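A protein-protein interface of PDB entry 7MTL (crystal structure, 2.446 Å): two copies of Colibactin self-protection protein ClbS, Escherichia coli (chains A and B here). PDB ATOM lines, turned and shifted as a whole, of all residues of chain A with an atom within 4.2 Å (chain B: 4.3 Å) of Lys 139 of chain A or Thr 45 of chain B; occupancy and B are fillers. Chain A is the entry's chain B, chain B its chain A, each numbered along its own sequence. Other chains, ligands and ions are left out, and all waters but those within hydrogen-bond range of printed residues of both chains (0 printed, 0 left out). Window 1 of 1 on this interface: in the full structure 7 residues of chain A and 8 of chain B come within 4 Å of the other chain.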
ATOM      1  N   TYR A 137       6.410  23.263  -5.299  1.00  0.00           N
ATOM      2  CA  TYR A 137       6.084  22.637  -6.574  1.00  0.00           C
ATOM      3  C   TYR A 137       4.950  23.436  -7.188  1.00  0.00           C
ATOM      4  O   TYR A 137       3.797  23.315  -6.752  1.00  0.00           O
ATOM      5  CB  TYR A 137       5.672  21.182  -6.409  1.00  0.00           C
ATOM      6  CG  TYR A 137       5.385  20.540  -7.733  1.00  0.00           C
ATOM      7  CD1 TYR A 137       6.364  20.473  -8.710  1.00  0.00           C
ATOM      8  CD2 TYR A 137       4.127  20.019  -8.024  1.00  0.00           C
ATOM      9  CE1 TYR A 137       6.103  19.895  -9.965  1.00  0.00           C
ATOM     10  CE2 TYR A 137       3.865  19.434  -9.251  1.00  0.00           C
ATOM     11  CZ  TYR A 137       4.863  19.375 -10.216  1.00  0.00           C
ATOM     12  OH  TYR A 137       4.612  18.790 -11.435  1.00  0.00           O
ATOM     13  N   ASN A 138       5.280  24.240  -8.192  1.00  0.00           N
ATOM     14  CA  ASN A 138       4.361  25.251  -8.708  1.00  0.00           C
ATOM     15  C   ASN A 138       3.938  26.071  -7.492  1.00  0.00           C
ATOM     16  O   ASN A 138       4.808  26.507  -6.726  1.00  0.00           O
ATOM     17  CB  ASN A 138       3.248  24.589  -9.501  1.00  0.00           C
ATOM     18  CG  ASN A 138       3.787  23.858 -10.711  1.00  0.00           C
ATOM     19  OD1 ASN A 138       4.546  24.425 -11.489  1.00  0.00           O
ATOM     20  ND2 ASN A 138       3.438  22.583 -10.852  1.00  0.00           N
ATOM     21  N   LYS A 139       2.662  26.293  -7.259  1.00  0.00           N
ATOM     22  CA  LYS A 139       2.315  27.068  -6.084  1.00  0.00           C
ATOM     23  C   LYS A 139       2.192  26.216  -4.821  1.00  0.00           C
ATOM     24  O   LYS A 139       2.035  26.775  -3.735  1.00  0.00           O
ATOM     25  CB  LYS A 139       1.018  27.843  -6.349  1.00  0.00           C
ATOM     26  CG  LYS A 139       1.055  28.651  -7.659  1.00  0.00           C
ATOM     27  CD  LYS A 139       2.118  29.743  -7.627  1.00  0.00           C
ATOM     28  CE  LYS A 139       2.468  30.273  -9.029  1.00  0.00           C
ATOM     29  NZ  LYS A 139       3.874  29.869  -9.442  1.00  0.00           N
ATOM     30  N   TRP A 140       2.254  24.892  -4.928  1.00  0.00           N
ATOM     31  CA  TRP A 140       2.008  24.035  -3.778  1.00  0.00           C
ATOM     32  C   TRP A 140       3.221  24.038  -2.850  1.00  0.00           C
ATOM     33  O   TRP A 140       4.356  23.808  -3.294  1.00  0.00           O
ATOM     34  CB  TRP A 140       1.677  22.611  -4.238  1.00  0.00           C
ATOM     35  CG  TRP A 140       0.484  22.597  -5.110  1.00  0.00           C
ATOM     36  CD1 TRP A 140       0.462  22.531  -6.481  1.00  0.00           C
ATOM     37  CD2 TRP A 140      -0.879  22.708  -4.690  1.00  0.00           C
ATOM     38  NE1 TRP A 140      -0.831  22.582  -6.931  1.00  0.00           N
ATOM     39  CE2 TRP A 140      -1.678  22.688  -5.858  1.00  0.00           C
ATOM     40  CE3 TRP A 140      -1.506  22.811  -3.436  1.00  0.00           C
ATOM     41  CZ2 TRP A 140      -3.076  22.770  -5.813  1.00  0.00           C
ATOM     42  CZ3 TRP A 140      -2.900  22.898  -3.385  1.00  0.00           C
ATOM     43  CH2 TRP A 140      -3.670  22.882  -4.573  1.00  0.00           C
ATOM     44  N   THR A 141       2.985  24.310  -1.566  1.00  0.00           N
ATOM     45  CA  THR A 141       4.077  24.321  -0.596  1.00  0.00           C
ATOM     46  C   THR A 141       4.612  22.910  -0.369  1.00  0.00           C
ATOM     47  O   THR A 141       3.899  21.914  -0.525  1.00  0.00           O
ATOM     48  CB  THR A 141       3.618  24.913   0.740  1.00  0.00           C
ATOM     49  OG1 THR A 141       2.593  24.088   1.319  1.00  0.00           O
ATOM     50  CG2 THR A 141       3.104  26.322   0.558  1.00  0.00           C
ATOM     51  N   LEU B  38       1.790  35.325  -0.487  1.00  0.00           N
ATOM     52  CA  LEU B  38       0.412  35.206  -0.052  1.00  0.00           C
ATOM     53  C   LEU B  38      -0.038  33.758  -0.054  1.00  0.00           C
ATOM     54  O   LEU B  38       0.286  32.992  -0.970  1.00  0.00           O
ATOM     55  CB  LEU B  38      -0.500  36.016  -0.961  1.00  0.00           C
ATOM     56  CG  LEU B  38      -0.136  37.475  -1.084  1.00  0.00           C
ATOM     57  CD1 LEU B  38      -1.162  38.128  -2.009  1.00  0.00           C
ATOM     58  CD2 LEU B  38      -0.140  38.054   0.306  1.00  0.00           C
ATOM     59  N   GLU B  39      -0.788  33.394   0.978  1.00  0.00           N
ATOM     60  CA  GLU B  39      -1.557  32.173   0.919  1.00  0.00           C
ATOM     61  C   GLU B  39      -2.528  32.300  -0.244  1.00  0.00           C
ATOM     62  O   GLU B  39      -3.181  33.335  -0.411  1.00  0.00           O
ATOM     63  CB  GLU B  39      -2.296  31.947   2.235  1.00  0.00           C
ATOM     64  CG  GLU B  39      -3.208  30.744   2.235  1.00  0.00           C
ATOM     65  CD  GLU B  39      -2.435  29.460   2.469  1.00  0.00           C
ATOM     66  OE1 GLU B  39      -1.184  29.484   2.405  1.00  0.00           O
ATOM     67  OE2 GLU B  39      -3.070  28.425   2.743  1.00  0.00           O
ATOM     68  N   GLY B  40      -2.596  31.264  -1.076  1.00  0.00           N
ATOM     69  CA  GLY B  40      -3.336  31.371  -2.310  1.00  0.00           C
ATOM     70  C   GLY B  40      -4.808  31.010  -2.188  1.00  0.00           C
ATOM     71  O   GLY B  40      -5.328  30.579  -1.160  1.00  0.00           O
ATOM     72  N   ALA B  42      -6.170  28.497  -3.147  1.00  0.00           N
ATOM     73  CA  ALA B  42      -6.236  27.124  -2.667  1.00  0.00           C
ATOM     74  C   ALA B  42      -5.310  26.934  -1.466  1.00  0.00           C
ATOM     75  O   ALA B  42      -4.172  27.422  -1.460  1.00  0.00           O
ATOM     76  CB  ALA B  42      -5.864  26.139  -3.778  1.00  0.00           C
ATOM     77  N   LYS B  43      -5.811  26.216  -0.455  1.00  0.00           N
ATOM     78  CA  LYS B  43      -5.076  26.034   0.795  1.00  0.00           C
ATOM     79  C   LYS B  43      -3.763  25.308   0.544  1.00  0.00           C
ATOM     80  O   LYS B  43      -3.719  24.314  -0.191  1.00  0.00           O
ATOM     81  CB  LYS B  43      -5.919  25.234   1.796  1.00  0.00           C
ATOM     82  CG  LYS B  43      -7.091  25.993   2.374  1.00  0.00           C
ATOM     83  CD  LYS B  43      -7.353  25.587   3.809  1.00  0.00           C
ATOM     84  CE  LYS B  43      -8.230  26.604   4.526  1.00  0.00           C
ATOM     85  NZ  LYS B  43      -9.610  26.561   4.013  1.00  0.00           N
ATOM     86  N   GLY B  44      -2.695  25.796   1.179  1.00  0.00           N
ATOM     87  CA  GLY B  44      -1.387  25.181   1.027  1.00  0.00           C
ATOM     88  C   GLY B  44      -0.619  25.626  -0.207  1.00  0.00           C
ATOM     89  O   GLY B  44       0.265  24.895  -0.693  1.00  0.00           O
ATOM     90  N   THR B  45      -0.937  26.806  -0.737  1.00  0.00           N
ATOM     91  CA  THR B  45      -0.213  27.391  -1.851  1.00  0.00           C
ATOM     92  C   THR B  45       0.321  28.750  -1.440  1.00  0.00           C
ATOM     93  O   THR B  45      -0.246  29.428  -0.583  1.00  0.00           O
ATOM     94  CB  THR B  45      -1.093  27.613  -3.097  1.00  0.00           C
ATOM     95  OG1 THR B  45      -2.081  28.595  -2.780  1.00  0.00           O
ATOM     96  CG2 THR B  45      -1.758  26.312  -3.611  1.00  0.00           C
ATOM     97  N   THR B  46       1.387  29.168  -2.110  1.00  0.00           N
ATOM     98  CA  THR B  46       1.918  30.513  -1.952  1.00  0.00           C
ATOM     99  C   THR B  46       1.964  31.183  -3.316  1.00  0.00           C
ATOM    100  O   THR B  46       2.501  30.613  -4.281  1.00  0.00           O
ATOM    101  CB  THR B  46       3.312  30.500  -1.307  1.00  0.00           C
ATOM    102  OG1 THR B  46       3.227  29.904   0.002  1.00  0.00           O
ATOM    103  CG2 THR B  46       3.820  31.899  -1.200  1.00  0.00           C
ATOM    104  N   ILE B  47       1.401  32.393  -3.394  1.00  0.00           N
ATOM    105  CA  ILE B  47       1.236  33.104  -4.653  1.00  0.00           C
ATOM    106  C   ILE B  47       1.656  34.554  -4.455  1.00  0.00           C
ATOM    107  O   ILE B  47       1.807  35.031  -3.327  1.00  0.00           O
ATOM    108  CB  ILE B  47      -0.215  33.025  -5.164  1.00  0.00           C
ATOM    109  CG1 ILE B  47      -1.137  33.795  -4.214  1.00  0.00           C
ATOM    110  CG2 ILE B  47      -0.649  31.576  -5.270  1.00  0.00           C
ATOM    111  CD1 ILE B  47      -2.544  33.986  -4.751  1.00  0.00           C
ATOM    112  N   ASN B  51      -0.039  36.817  -9.305  1.00  0.00           N
ATOM    113  CA  ASN B  51      -0.974  35.702  -9.450  1.00  0.00           C
ATOM    114  C   ASN B  51      -2.393  36.116  -9.054  1.00  0.00           C
ATOM    115  O   ASN B  51      -3.381  35.655  -9.643  1.00  0.00           O
ATOM    116  CB  ASN B  51      -0.538  34.507  -8.602  1.00  0.00           C
ATOM    117  CG  ASN B  51       0.884  34.106  -8.845  1.00  0.00           C
ATOM    118  OD1 ASN B  51       1.634  33.850  -7.898  1.00  0.00           O
ATOM    119  ND2 ASN B  51       1.271  34.026 -10.098  1.00  0.00           N
ATOM    120  N   GLN B  93      -5.112  27.632 -10.540  1.00  0.00           N
ATOM    121  CA  GLN B  93      -3.726  27.374 -10.933  1.00  0.00           C
ATOM    122  C   GLN B  93      -3.544  27.599 -12.420  1.00  0.00           C
ATOM    123  O   GLN B  93      -2.576  28.244 -12.847  1.00  0.00           O
ATOM    124  CB  GLN B  93      -3.310  25.947 -10.558  1.00  0.00           C
ATOM    125  CG  GLN B  93      -3.842  25.498  -9.214  1.00  0.00           C
ATOM    126  CD  GLN B  93      -3.236  26.309  -8.039  1.00  0.00           C
ATOM    127  OE1 GLN B  93      -2.035  26.537  -7.982  1.00  0.00           O
ATOM    128  NE2 GLN B  93      -4.080  26.746  -7.129  1.00  0.00           N
ATOM    129  N   TYR B  96      -3.148  31.181 -12.940  1.00  0.00           N
ATOM    130  CA  TYR B  96      -1.808  31.716 -12.691  1.00  0.00           C
ATOM    131  C   TYR B  96      -0.911  31.441 -13.880  1.00  0.00           C
ATOM    132  O   TYR B  96      -0.237  32.344 -14.383  1.00  0.00           O
ATOM    133  CB  TYR B  96      -1.145  31.141 -11.424  1.00  0.00           C
ATOM    134  CG  TYR B  96      -1.986  31.141 -10.195  1.00  0.00           C
ATOM    135  CD1 TYR B  96      -2.821  32.210  -9.903  1.00  0.00           C
ATOM    136  CD2 TYR B  96      -1.959  30.059  -9.324  1.00  0.00           C
ATOM    137  CE1 TYR B  96      -3.605  32.199  -8.749  1.00  0.00           C
ATOM    138  CE2 TYR B  96      -2.728  30.045  -8.183  1.00  0.00           C
ATOM    139  CZ  TYR B  96      -3.546  31.116  -7.895  1.00  0.00           C
ATOM    140  OH  TYR B  96      -4.327  31.103  -6.760  1.00  0.00           O
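The backbone carbonyl oxygen of Gly 44 of chain B lies within hydrogen-bond range of the backbone NH of Thr 141 of chain A.
N of Thr 46 of chain B lies within hydrogen-bond range of O of Lys 139 of chain A, at 3.0 Å.
The backbone NH of Gly 40 of chain B lies within hydrogen-bond range of the backbone carbonyl oxygen of Thr 45 of chain B.
The side-chain hydroxyl (OG1) of Thr 45 of chain B lies within hydrogen-bond range of the backbone carbonyl oxygen (O) of Ala 42 of chain B, at 2.7 Å.
The side-chain carboxylate (OE2) of Glu 39 of chain B sits at hydrogen-bond distance from the backbone NH (N) of Gly 44 of chain B (3.1 Å).
Lys 139 of chain A touches Gly 44 of chain B (O to O, 3.99 Å).
Lys 139 of chain A touches Thr 45 of chain B (O to CA, 3.0 Å).
Lys 139 of chain A touches Asn 51 of chain B.
Lys 139 of chain A touches Gln 93 of chain B.
Tyr 96 of chain B touches Lys 139 of chain A.
Lys 43 of chain B touches Trp 140 of chain A.
Trp 140 of chain A touches Gly 44 of chain B.
Thr 45 of chain B touches Trp 140 of chain A (CG2 to CE3, 3.5 Å).
CG2 of Thr 141 of chain A touches OG1 of Thr 46 of chain B, 3.6 Å away.
Of the printed residues of chain B, Lys 139 of chain A touches Gly 44 (3.99 Å), Thr 45 (3.0 Å), Thr 46 (3.0 Å), Asn 51 (3.8 Å), Gln 93 (3.7 Å) and Tyr 96 (3.7 Å).
Of the printed residues of chain B, Thr 141 of chain A touches Gly 44 and Thr 46.
Of the printed residues of chain A, Lys 43 of chain B touches Trp 140 (3.6 Å).
Printed residues of chain A within 4 Å of Thr 46 of chain B: Lys 139 and Thr 141.
Printed residues of chain A within 4 Å of Asn 51 of chain B: Lys 139 (3.8 Å).
Of the printed residues of chain A, Tyr 96 of chain B touches Lys 139.
The nearest printed residue of chain B that does not touch Lys 139 of chain A is Ile 47 of chain B (4.1 Å).
The nearest printed residue of chain A that does not touch Tyr 96 of chain B is Asn 138 of chain A (7.4 Å).
Of the 12 printed residues of chain B, 7 touch a printed residue of chain A.
Hydrophobic or aromatic side chains of chain B within 4 Å of the printed part of chain A: Tyr 96.
Of the 5 printed residues of chain A, 3 touch a printed residue of chain B.
Printed residues of chain A that touch a printed residue of chain B: Lys 139, Trp 140 and Thr 141.
Hydrophobic or aromatic side chains of chain A within 4 Å of the printed part of chain B: Trp 140.
Along chain A the printed residues that touch a printed residue of chain B span positions 139 to 141.
Among the printed residues, no Asp or Glu carboxylate lies within 4 Å of a Lys or Arg side-chain nitrogen of the other chain.
No position is printed for both chains.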
